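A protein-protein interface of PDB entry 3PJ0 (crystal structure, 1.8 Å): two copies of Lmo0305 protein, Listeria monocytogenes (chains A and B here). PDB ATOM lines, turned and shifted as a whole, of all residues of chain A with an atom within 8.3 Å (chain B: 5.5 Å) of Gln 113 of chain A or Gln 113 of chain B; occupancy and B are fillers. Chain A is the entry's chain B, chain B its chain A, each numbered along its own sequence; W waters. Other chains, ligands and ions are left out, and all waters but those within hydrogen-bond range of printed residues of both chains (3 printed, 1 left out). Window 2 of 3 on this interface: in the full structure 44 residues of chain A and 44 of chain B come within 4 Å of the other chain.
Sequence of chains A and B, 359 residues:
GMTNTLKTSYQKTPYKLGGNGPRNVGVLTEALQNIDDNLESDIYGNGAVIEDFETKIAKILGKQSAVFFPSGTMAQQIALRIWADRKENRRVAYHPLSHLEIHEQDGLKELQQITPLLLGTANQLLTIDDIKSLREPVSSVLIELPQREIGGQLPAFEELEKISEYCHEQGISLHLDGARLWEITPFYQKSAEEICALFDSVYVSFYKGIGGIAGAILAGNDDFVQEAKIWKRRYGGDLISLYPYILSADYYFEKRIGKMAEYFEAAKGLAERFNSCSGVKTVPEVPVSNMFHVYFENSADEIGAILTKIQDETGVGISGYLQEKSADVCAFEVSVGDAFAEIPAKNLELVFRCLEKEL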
ATOM      1  N   GLN A  77      16.580  20.963 -12.442  1.00  0.00           N
ATOM      2  CA  GLN A  77      16.855  20.425 -11.117  1.00  0.00           C
ATOM      3  C   GLN A  77      18.296  20.724 -10.701  1.00  0.00           C
ATOM      4  O   GLN A  77      18.572  21.085  -9.559  1.00  0.00           O
ATOM      5  CB  GLN A  77      16.663  18.905 -11.110  1.00  0.00           C
ATOM      6  CG  GLN A  77      15.214  18.510 -11.230  1.00  0.00           C
ATOM      7  CD  GLN A  77      15.018  17.005 -11.154  1.00  0.00           C
ATOM      8  OE1 GLN A  77      15.770  16.301 -10.470  1.00  0.00           O
ATOM      9  NE2 GLN A  77      13.951  16.519 -11.784  1.00  0.00           N
ATOM     10  N   ARG A  81      19.891  23.153  -7.700  1.00  0.00           N
ATOM     11  CA  ARG A  81      20.803  22.579  -6.696  1.00  0.00           C
ATOM     12  C   ARG A  81      22.110  23.399  -6.598  1.00  0.00           C
ATOM     13  O   ARG A  81      22.602  23.692  -5.510  1.00  0.00           O
ATOM     14  CB  ARG A  81      21.136  21.145  -7.010  1.00  0.00           C
ATOM     15  CG  ARG A  81      22.215  20.518  -6.095  1.00  0.00           C
ATOM     16  CD  ARG A  81      21.812  20.556  -4.610  1.00  0.00           C
ATOM     17  NE  ARG A  81      22.852  19.977  -3.772  1.00  0.00           N
ATOM     18  CZ  ARG A  81      22.938  18.691  -3.430  1.00  0.00           C
ATOM     19  NH1 ARG A  81      22.009  17.796  -3.830  1.00  0.00           N
ATOM     20  NH2 ARG A  81      23.955  18.296  -2.651  1.00  0.00           N
ATOM     21  N   ALA A  84      21.415  26.509  -4.774  1.00  0.00           N
ATOM     22  CA  ALA A  84      21.121  26.107  -3.393  1.00  0.00           C
ATOM     23  C   ALA A  84      22.412  25.861  -2.605  1.00  0.00           C
ATOM     24  O   ALA A  84      22.546  26.288  -1.438  1.00  0.00           O
ATOM     25  CB  ALA A  84      20.202  24.849  -3.378  1.00  0.00           C
ATOM     26  N   ASN A  89      21.139  27.164   1.018  1.00  0.00           N
ATOM     27  CA  ASN A  89      19.700  27.354   1.284  1.00  0.00           C
ATOM     28  C   ASN A  89      18.923  26.500   0.286  1.00  0.00           C
ATOM     29  O   ASN A  89      18.959  26.757  -0.918  1.00  0.00           O
ATOM     30  CB  ASN A  89      19.376  28.844   1.158  1.00  0.00           C
ATOM     31  CG  ASN A  89      17.910  29.189   1.448  1.00  0.00           C
ATOM     32  OD1 ASN A  89      17.011  28.358   1.343  1.00  0.00           O
ATOM     33  ND2 ASN A  89      17.678  30.428   1.846  1.00  0.00           N
ATOM     34  N   ARG A  90      18.221  25.484   0.787  1.00  0.00           N
ATOM     35  CA  ARG A  90      17.513  24.546  -0.097  1.00  0.00           C
ATOM     36  C   ARG A  90      16.065  24.951  -0.412  1.00  0.00           C
ATOM     37  O   ARG A  90      15.293  24.146  -0.932  1.00  0.00           O
ATOM     38  CB  ARG A  90      17.550  23.120   0.491  1.00  0.00           C
ATOM     39  CG  ARG A  90      18.929  22.487   0.519  1.00  0.00           C
ATOM     40  CD  ARG A  90      19.354  21.857  -0.842  1.00  0.00           C
ATOM     41  NE  ARG A  90      20.672  21.281  -0.614  1.00  0.00           N
ATOM     42  CZ  ARG A  90      20.986  19.981  -0.577  1.00  0.00           C
ATOM     43  NH1 ARG A  90      20.110  19.025  -0.870  1.00  0.00           N
ATOM     44  NH2 ARG A  90      22.208  19.639  -0.211  1.00  0.00           N
ATOM     45  N   ARG A  91      15.691  26.178  -0.096  1.00  0.00           N
ATOM     46  CA  ARG A  91      14.367  26.682  -0.472  1.00  0.00           C
ATOM     47  C   ARG A  91      14.490  27.443  -1.773  1.00  0.00           C
ATOM     48  O   ARG A  91      15.470  28.164  -1.949  1.00  0.00           O
ATOM     49  CB  ARG A  91      13.784  27.611   0.575  1.00  0.00           C
ATOM     50  CG  ARG A  91      13.353  26.911   1.863  1.00  0.00           C
ATOM     51  CD  ARG A  91      12.529  27.802   2.748  1.00  0.00           C
ATOM     52  NE  ARG A  91      13.259  28.982   3.216  1.00  0.00           N
ATOM     53  CZ  ARG A  91      13.965  29.061   4.336  1.00  0.00           C
ATOM     54  NH1 ARG A  91      14.122  27.998   5.122  1.00  0.00           N
ATOM     55  NH2 ARG A  91      14.547  30.215   4.661  1.00  0.00           N
ATOM     56  N   ASP A 106       7.907  14.890  -8.966  1.00  0.00           N
ATOM     57  CA  ASP A 106       8.522  15.396  -7.751  1.00  0.00           C
ATOM     58  C   ASP A 106      10.056  15.203  -7.676  1.00  0.00           C
ATOM     59  O   ASP A 106      10.616  15.132  -6.592  1.00  0.00           O
ATOM     60  CB  ASP A 106       7.862  14.758  -6.522  1.00  0.00           C
ATOM     61  CG  ASP A 106       6.330  14.753  -6.597  1.00  0.00           C
ATOM     62  OD1 ASP A 106       5.693  15.833  -6.740  1.00  0.00           O
ATOM     63  OD2 ASP A 106       5.780  13.647  -6.453  1.00  0.00           O
ATOM     64  N   GLY A 107      10.729  15.158  -8.822  1.00  0.00           N
ATOM     65  CA  GLY A 107      12.174  15.011  -8.885  1.00  0.00           C
ATOM     66  C   GLY A 107      12.991  15.999  -8.064  1.00  0.00           C
ATOM     67  O   GLY A 107      13.938  15.609  -7.365  1.00  0.00           O
ATOM     68  N   LEU A 108      12.632  17.276  -8.151  1.00  0.00           N
ATOM     69  CA  LEU A 108      13.327  18.313  -7.402  1.00  0.00           C
ATOM     70  C   LEU A 108      13.284  17.991  -5.912  1.00  0.00           C
ATOM     71  O   LEU A 108      14.285  18.104  -5.217  1.00  0.00           O
ATOM     72  CB  LEU A 108      12.684  19.674  -7.644  1.00  0.00           C
ATOM     73  CG  LEU A 108      13.312  20.931  -7.032  1.00  0.00           C
ATOM     74  CD1 LEU A 108      14.753  21.146  -7.557  1.00  0.00           C
ATOM     75  CD2 LEU A 108      12.409  22.170  -7.268  1.00  0.00           C
ATOM     76  N   LYS A 109      12.097  17.632  -5.431  1.00  0.00           N
ATOM     77  CA  LYS A 109      11.936  17.318  -4.017  1.00  0.00           C
ATOM     78  C   LYS A 109      12.647  16.035  -3.640  1.00  0.00           C
ATOM     79  O   LYS A 109      13.332  15.964  -2.608  1.00  0.00           O
ATOM     80  CB  LYS A 109      10.464  17.235  -3.644  1.00  0.00           C
ATOM     81  CG  LYS A 109       9.695  18.536  -3.815  1.00  0.00           C
ATOM     82  CD  LYS A 109       8.162  18.349  -3.717  1.00  0.00           C
ATOM     83  CE  LYS A 109       7.454  19.647  -4.080  1.00  0.00           C
ATOM     84  NZ  LYS A 109       5.974  19.552  -4.053  1.00  0.00           N
ATOM     85  N   GLU A 110      12.517  15.032  -4.493  1.00  0.00           N
ATOM     86  CA  GLU A 110      12.991  13.700  -4.154  1.00  0.00           C
ATOM     87  C   GLU A 110      14.469  13.478  -4.378  1.00  0.00           C
ATOM     88  O   GLU A 110      15.115  12.767  -3.586  1.00  0.00           O
ATOM     89  CB  GLU A 110      12.199  12.650  -4.937  1.00  0.00           C
ATOM     90  CG  GLU A 110      10.747  12.534  -4.553  1.00  0.00           C
ATOM     91  CD  GLU A 110      10.473  11.895  -3.200  1.00  0.00           C
ATOM     92  OE1 GLU A 110      11.408  11.403  -2.503  1.00  0.00           O
ATOM     93  OE2 GLU A 110       9.272  11.901  -2.837  1.00  0.00           O
ATOM     94  N   LEU A 111      15.003  14.043  -5.451  1.00  0.00           N
ATOM     95  CA  LEU A 111      16.407  13.904  -5.771  1.00  0.00           C
ATOM     96  C   LEU A 111      17.318  14.978  -5.175  1.00  0.00           C
ATOM     97  O   LEU A 111      18.441  14.675  -4.779  1.00  0.00           O
ATOM     98  CB  LEU A 111      16.611  13.856  -7.285  1.00  0.00           C
ATOM     99  CG  LEU A 111      16.092  12.581  -7.936  1.00  0.00           C
ATOM    100  CD1 LEU A 111      16.184  12.759  -9.481  1.00  0.00           C
ATOM    101  CD2 LEU A 111      16.875  11.324  -7.452  1.00  0.00           C
ATOM    102  N   GLN A 112      16.838  16.221  -5.121  1.00  0.00           N
ATOM    103  CA  GLN A 112      17.624  17.360  -4.663  1.00  0.00           C
ATOM    104  C   GLN A 112      17.323  17.856  -3.252  1.00  0.00           C
ATOM    105  O   GLN A 112      17.997  18.755  -2.772  1.00  0.00           O
ATOM    106  CB  GLN A 112      17.457  18.532  -5.657  1.00  0.00           C
ATOM    107  CG  GLN A 112      18.099  18.238  -7.018  1.00  0.00           C
ATOM    108  CD  GLN A 112      19.555  17.889  -6.885  1.00  0.00           C
ATOM    109  OE1 GLN A 112      20.204  18.259  -5.900  1.00  0.00           O
ATOM    110  NE2 GLN A 112      20.090  17.160  -7.876  1.00  0.00           N
ATOM    111  N   GLN A 113      16.324  17.277  -2.588  1.00  0.00           N
ATOM    112  CA  GLN A 113      15.975  17.677  -1.205  1.00  0.00           C
ATOM    113  C   GLN A 113      15.828  19.200  -1.114  1.00  0.00           C
ATOM    114  O   GLN A 113      16.392  19.839  -0.228  1.00  0.00           O
ATOM    115  CB  GLN A 113      16.976  17.081  -0.196  1.00  0.00           C
ATOM    116  CG  GLN A 113      16.983  15.527  -0.315  1.00  0.00           C
ATOM    117  CD  GLN A 113      17.866  14.784   0.672  1.00  0.00           C
ATOM    118  OE1 GLN A 113      18.916  15.274   1.101  1.00  0.00           O
ATOM    119  NE2 GLN A 113      17.448  13.563   1.016  1.00  0.00           N
ATOM    120  N   ILE A 114      15.081  19.760  -2.074  1.00  0.00           N
ATOM    121  CA  ILE A 114      14.748  21.189  -2.142  1.00  0.00           C
ATOM    122  C   ILE A 114      13.270  21.397  -1.787  1.00  0.00           C
ATOM    123  O   ILE A 114      12.420  20.571  -2.126  1.00  0.00           O
ATOM    124  CB  ILE A 114      15.112  21.783  -3.531  1.00  0.00           C
ATOM    125  CG1 ILE A 114      16.620  22.042  -3.558  1.00  0.00           C
ATOM    126  CG2 ILE A 114      14.313  23.102  -3.832  1.00  0.00           C
ATOM    127  CD1 ILE A 114      17.194  22.395  -4.910  1.00  0.00           C
ATOM    128  N   THR A 115      12.983  22.497  -1.094  1.00  0.00           N
ATOM    129  CA  THR A 115      11.646  22.852  -0.667  1.00  0.00           C
ATOM    130  C   THR A 115      11.169  24.047  -1.459  1.00  0.00           C
ATOM    131  O   THR A 115      11.639  25.156  -1.240  1.00  0.00           O
ATOM    132  CB  THR A 115      11.638  23.173   0.850  1.00  0.00           C
ATOM    133  OG1 THR A 115      11.970  21.984   1.566  1.00  0.00           O
ATOM    134  CG2 THR A 115      10.267  23.633   1.327  1.00  0.00           C
ATOM    135  N   PRO A 116      10.236  23.822  -2.408  1.00  0.00           N
ATOM    136  CA  PRO A 116       9.759  24.935  -3.189  1.00  0.00           C
ATOM    137  C   PRO A 116       8.596  25.690  -2.548  1.00  0.00           C
ATOM    138  O   PRO A 116       7.610  25.072  -2.121  1.00  0.00           O
ATOM    139  CB  PRO A 116       9.313  24.271  -4.533  1.00  0.00           C
ATOM    140  CG  PRO A 116       9.742  22.864  -4.461  1.00  0.00           C
ATOM    141  CD  PRO A 116       9.835  22.534  -3.009  1.00  0.00           C
ATOM    142  N   TRP A 231      27.088  17.256 -12.119  1.00  0.00           N
ATOM    143  CA  TRP A 231      25.739  16.747 -11.844  1.00  0.00           C
ATOM    144  C   TRP A 231      25.167  15.937 -13.024  1.00  0.00           C
ATOM    145  O   TRP A 231      24.489  14.944 -12.800  1.00  0.00           O
ATOM    146  CB  TRP A 231      24.766  17.863 -11.447  1.00  0.00           C
ATOM    147  CG  TRP A 231      24.951  18.366 -10.049  1.00  0.00           C
ATOM    148  CD1 TRP A 231      25.528  19.540  -9.662  1.00  0.00           C
ATOM    149  CD2 TRP A 231      24.581  17.682  -8.846  1.00  0.00           C
ATOM    150  NE1 TRP A 231      25.519  19.635  -8.283  1.00  0.00           N
ATOM    151  CE2 TRP A 231      24.942  18.506  -7.766  1.00  0.00           C
ATOM    152  CE3 TRP A 231      23.965  16.452  -8.584  1.00  0.00           C
ATOM    153  CZ2 TRP A 231      24.740  18.126  -6.435  1.00  0.00           C
ATOM    154  CZ3 TRP A 231      23.756  16.085  -7.260  1.00  0.00           C
ATOM    155  CH2 TRP A 231      24.136  16.922  -6.209  1.00  0.00           C
ATOM    156  N   TYR A 235      23.482  12.233 -12.779  1.00  0.00           N
ATOM    157  CA  TYR A 235      22.138  11.941 -13.249  1.00  0.00           C
ATOM    158  C   TYR A 235      22.047  10.874 -14.340  1.00  0.00           C
ATOM    159  O   TYR A 235      20.941  10.413 -14.645  1.00  0.00           O
ATOM    160  CB  TYR A 235      21.435  13.210 -13.763  1.00  0.00           C
ATOM    161  CG  TYR A 235      20.668  14.013 -12.741  1.00  0.00           C
ATOM    162  CD1 TYR A 235      21.309  14.848 -11.830  1.00  0.00           C
ATOM    163  CD2 TYR A 235      19.280  13.905 -12.661  1.00  0.00           C
ATOM    164  CE1 TYR A 235      20.572  15.602 -10.926  1.00  0.00           C
ATOM    165  CE2 TYR A 235      18.560  14.620 -11.769  1.00  0.00           C
ATOM    166  CZ  TYR A 235      19.199  15.489 -10.907  1.00  0.00           C
ATOM    167  OH  TYR A 235      18.454  16.180  -9.990  1.00  0.00           O
ATOM    168  N   ARG B  81      17.976   1.902  -5.656  1.00  0.00           N
ATOM    169  CA  ARG B  81      16.989   2.643  -4.829  1.00  0.00           C
ATOM    170  C   ARG B  81      15.661   1.887  -4.644  1.00  0.00           C
ATOM    171  O   ARG B  81      15.103   1.838  -3.546  1.00  0.00           O
ATOM    172  CB  ARG B  81      16.738   4.059  -5.382  1.00  0.00           C
ATOM    173  CG  ARG B  81      15.664   4.872  -4.591  1.00  0.00           C
ATOM    174  CD  ARG B  81      15.994   5.051  -3.124  1.00  0.00           C
ATOM    175  NE  ARG B  81      14.879   5.722  -2.464  1.00  0.00           N
ATOM    176  CZ  ARG B  81      14.718   7.042  -2.388  1.00  0.00           C
ATOM    177  NH1 ARG B  81      15.637   7.881  -2.858  1.00  0.00           N
ATOM    178  NH2 ARG B  81      13.617   7.524  -1.814  1.00  0.00           N
ATOM    179  N   ARG B  90      19.247   1.298   3.125  1.00  0.00           N
ATOM    180  CA  ARG B  90      20.034   2.076   2.139  1.00  0.00           C
ATOM    181  C   ARG B  90      21.473   1.612   1.966  1.00  0.00           C
ATOM    182  O   ARG B  90      22.283   2.311   1.327  1.00  0.00           O
ATOM    183  CB  ARG B  90      19.979   3.590   2.466  1.00  0.00           C
ATOM    184  CG  ARG B  90      18.593   4.245   2.280  1.00  0.00           C
ATOM    185  CD  ARG B  90      18.218   4.679   0.865  1.00  0.00           C
ATOM    186  NE  ARG B  90      16.935   5.381   0.899  1.00  0.00           N
ATOM    187  CZ  ARG B  90      16.704   6.671   0.712  1.00  0.00           C
ATOM    188  NH1 ARG B  90      17.640   7.524   0.288  1.00  0.00           N
ATOM    189  NH2 ARG B  90      15.452   7.104   0.872  1.00  0.00           N
ATOM    190  N   LEU B 108      25.342   7.660  -7.004  1.00  0.00           N
ATOM    191  CA  LEU B 108      24.567   6.779  -6.085  1.00  0.00           C
ATOM    192  C   LEU B 108      24.552   7.343  -4.674  1.00  0.00           C
ATOM    193  O   LEU B 108      23.505   7.400  -4.018  1.00  0.00           O
ATOM    194  CB  LEU B 108      25.144   5.372  -6.099  1.00  0.00           C
ATOM    195  CG  LEU B 108      24.452   4.321  -5.221  1.00  0.00           C
ATOM    196  CD1 LEU B 108      23.006   4.071  -5.718  1.00  0.00           C
ATOM    197  CD2 LEU B 108      25.336   3.045  -5.239  1.00  0.00           C
ATOM    198  N   LYS B 109      25.709   7.786  -4.209  1.00  0.00           N
ATOM    199  CA  LYS B 109      25.831   8.428  -2.893  1.00  0.00           C
ATOM    200  C   LYS B 109      25.117   9.791  -2.809  1.00  0.00           C
ATOM    201  O   LYS B 109      24.394  10.084  -1.840  1.00  0.00           O
ATOM    202  CB  LYS B 109      27.312   8.601  -2.568  1.00  0.00           C
ATOM    203  CG  LYS B 109      28.048   7.229  -2.425  1.00  0.00           C
ATOM    204  CD  LYS B 109      29.535   7.398  -2.287  1.00  0.00           C
ATOM    205  CE  LYS B 109      30.270   6.017  -2.365  1.00  0.00           C
ATOM    206  NZ  LYS B 109      31.755   6.212  -2.425  1.00  0.00           N
ATOM    207  N   GLU B 110      25.306  10.621  -3.823  1.00  0.00           N
ATOM    208  CA  GLU B 110      24.821  12.007  -3.780  1.00  0.00           C
ATOM    209  C   GLU B 110      23.341  12.153  -4.099  1.00  0.00           C
ATOM    210  O   GLU B 110      22.688  13.065  -3.571  1.00  0.00           O
ATOM    211  CB  GLU B 110      25.619  12.891  -4.742  1.00  0.00           C
ATOM    212  CG  GLU B 110      27.114  13.010  -4.438  1.00  0.00           C
ATOM    213  CD  GLU B 110      27.472  14.001  -3.339  1.00  0.00           C
ATOM    214  OE1 GLU B 110      26.587  14.489  -2.577  1.00  0.00           O
ATOM    215  OE2 GLU B 110      28.683  14.290  -3.240  1.00  0.00           O
ATOM    216  N   LEU B 111      22.822  11.311  -4.993  1.00  0.00           N
ATOM    217  CA  LEU B 111      21.430  11.392  -5.402  1.00  0.00           C
ATOM    218  C   LEU B 111      20.518  10.439  -4.620  1.00  0.00           C
ATOM    219  O   LEU B 111      19.335  10.730  -4.420  1.00  0.00           O
ATOM    220  CB  LEU B 111      21.275  11.162  -6.905  1.00  0.00           C
ATOM    221  CG  LEU B 111      21.781  12.283  -7.830  1.00  0.00           C
ATOM    222  CD1 LEU B 111      21.759  11.838  -9.273  1.00  0.00           C
ATOM    223  CD2 LEU B 111      20.972  13.598  -7.617  1.00  0.00           C
ATOM    224  N   GLN B 112      21.069   9.323  -4.145  1.00  0.00           N
ATOM    225  CA  GLN B 112      20.235   8.338  -3.457  1.00  0.00           C
ATOM    226  C   GLN B 112      20.602   8.151  -1.981  1.00  0.00           C
ATOM    227  O   GLN B 112      19.892   7.452  -1.244  1.00  0.00           O
ATOM    228  CB  GLN B 112      20.288   6.995  -4.206  1.00  0.00           C
ATOM    229  CG  GLN B 112      19.682   6.986  -5.607  1.00  0.00           C
ATOM    230  CD  GLN B 112      18.216   7.388  -5.616  1.00  0.00           C
ATOM    231  OE1 GLN B 112      17.518   7.251  -4.619  1.00  0.00           O
ATOM    232  NE2 GLN B 112      17.754   7.911  -6.735  1.00  0.00           N
ATOM    233  N   GLN B 113      21.685   8.786  -1.530  1.00  0.00           N
ATOM    234  CA  GLN B 113      22.144   8.626  -0.137  1.00  0.00           C
ATOM    235  C   GLN B 113      22.206   7.143   0.247  1.00  0.00           C
ATOM    236  O   GLN B 113      21.850   6.753   1.370  1.00  0.00           O
ATOM    237  CB  GLN B 113      21.273   9.389   0.877  1.00  0.00           C
ATOM    238  CG  GLN B 113      21.317  10.885   0.710  1.00  0.00           C
ATOM    239  CD  GLN B 113      20.360  11.340  -0.317  1.00  0.00           C
ATOM    240  OE1 GLN B 113      19.199  10.931  -0.302  1.00  0.00           O
ATOM    241  NE2 GLN B 113      20.806  12.216  -1.205  1.00  0.00           N
ATOM    242  N   ILE B 114      22.653   6.335  -0.714  1.00  0.00           N
ATOM    243  CA  ILE B 114      22.907   4.914  -0.515  1.00  0.00           C
ATOM    244  C   ILE B 114      24.387   4.736  -0.133  1.00  0.00           C
ATOM    245  O   ILE B 114      25.275   5.437  -0.656  1.00  0.00           O
ATOM    246  CB  ILE B 114      22.493   4.115  -1.756  1.00  0.00           C
ATOM    247  CG1 ILE B 114      20.962   3.978  -1.748  1.00  0.00           C
ATOM    248  CG2 ILE B 114      23.260   2.727  -1.848  1.00  0.00           C
ATOM    249  CD1 ILE B 114      20.339   3.260  -2.980  1.00  0.00           C
ATOM    250  N   THR B 115      24.652   3.817   0.798  1.00  0.00           N
ATOM    251  CA  THR B 115      26.014   3.587   1.319  1.00  0.00           C
ATOM    252  C   THR B 115      26.509   2.254   0.787  1.00  0.00           C
ATOM    253  O   THR B 115      25.979   1.217   1.194  1.00  0.00           O
ATOM    254  CB  THR B 115      26.032   3.509   2.881  1.00  0.00           C
ATOM    255  OG1 THR B 115      25.599   4.753   3.469  1.00  0.00           O
ATOM    256  CG2 THR B 115      27.435   3.166   3.398  1.00  0.00           C
HETATM  257  O   HOH W   1      24.071  15.253  -2.418  1.00  0.00           O
HETATM  258  O   HOH W   2      16.724  10.527  -3.437  1.00  0.00           O
HETATM  259  O   HOH W   3      20.849  15.104  -3.569  1.00  0.00           O
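Of the 10 printed residues of chain B, 3 touch a printed residue of chain A. Printed residues of chain B that touch a printed residue of chain A: Leu 111, Gln 112 and Gln 113. Among the printed residues, 6 pairs touch across the chains. Among the printed residues, no Asp or Glu carboxylate lies within 4 Å of a Lys or Arg side-chain nitrogen of the other chain.
Water W1 bridges OE1 of Glu 110 of chain B and NH2 of Arg 81 of chain A. Water W3 lies within hydrogen-bond range of O of Leu 111 of chain A (2.7 Å), O of Glu 110 of chain B (2.7 Å) and NH1 of Arg 81 of chain A (2.9 Å). Water W2 lies within hydrogen-bond range of the backbone carbonyl oxygen of Glu 110 of chain A (2.8 Å), the backbone carbonyl oxygen of Leu 111 of chain B (2.8 Å) and the guanidinium group of Arg 81 of chain B (2.9 Å).
OE1 of Gln 113 of chain B lies within hydrogen-bond range of NE2 of Gln 113 of chain A, at 3.4 Å.
The guanidinium group (NH1) of Arg 81 of chain B lies within hydrogen-bond range of the side-chain amide oxygen (OE1) of Gln 112 of chain B (2.7 Å). The side-chain amide nitrogen (NE2) of Gln 112 of chain A lies within hydrogen-bond range of the side-chain hydroxyl (OH) of Tyr 235 of chain A, at 2.8 Å. NH1 of Arg 90 of chain A sits at hydrogen-bond distance from O of Gln 112 of chain A, at 2.9 Å. The guanidinium group of Arg 81 of chain A sits at hydrogen-bond distance from the side-chain amide oxygen of Gln 112 of chain A (2.8 Å). O of Glu 110 of chain B lies within hydrogen-bond range of NE2 of Gln 113 of chain B (3.1 Å). OE1 of Gln 77 of chain A is in hydrogen-bond range of OH of Tyr 235 of chain A (2.7 Å).
Gln 113 of chain A touches just one residue of chain B: Gln 113 (3.4 Å). Printed residues of chain B within 4 Å of Leu 111 of chain A: Leu 111 (3.9 Å) and Gln 112 (3.6 Å). Printed residues of chain B within 4 Å of Tyr 235 of chain A: Leu 111. Of the printed residues of chain A, Gln 112 of chain B touches Leu 111. Printed residues of chain A within 4 Å of Leu 111 of chain B: Leu 111 (3.9 Å), Gln 112 (3.7 Å), Trp 231 (3.8 Å) and Tyr 235 (3.9 Å). Printed residues of chain B within 4 Å of Trp 231 of chain A: Leu 111 (3.8 Å). Glu 110 of chain A touches none of the printed residues of chain B. The nearest printed residue of chain B that does not touch Gln 113 of chain A is Arg 90 of chain B (6.1 Å). The nearest printed residue of chain B that does not touch Trp 231 of chain A is Glu 110 of chain B (4.5 Å).
Leu 111 of chain B touches its own counterpart, Leu 111 of chain A. Leu 111 of chain A touches Gln 112 of chain B, and with the chains exchanged Gln 112 of chain A touches Leu 111 of chain B. Gln 113 of chain B touches its own counterpart, Gln 113 of chain A. Positions printed for both chains: 81, 90, 108, 109, 110, 111, 112, 113, 114 and 115.
Among the printed residues, merely in contact across the chains: Leu 111 of chain A with Gln 112 of chain B, Gln 112 of chain A with Leu 111 of chain B, Trp 231 of chain A with Leu 111 of chain B, Tyr 235 of chain A with Leu 111 of chain B and Leu 111 of chain A with Leu 111 of chain B.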
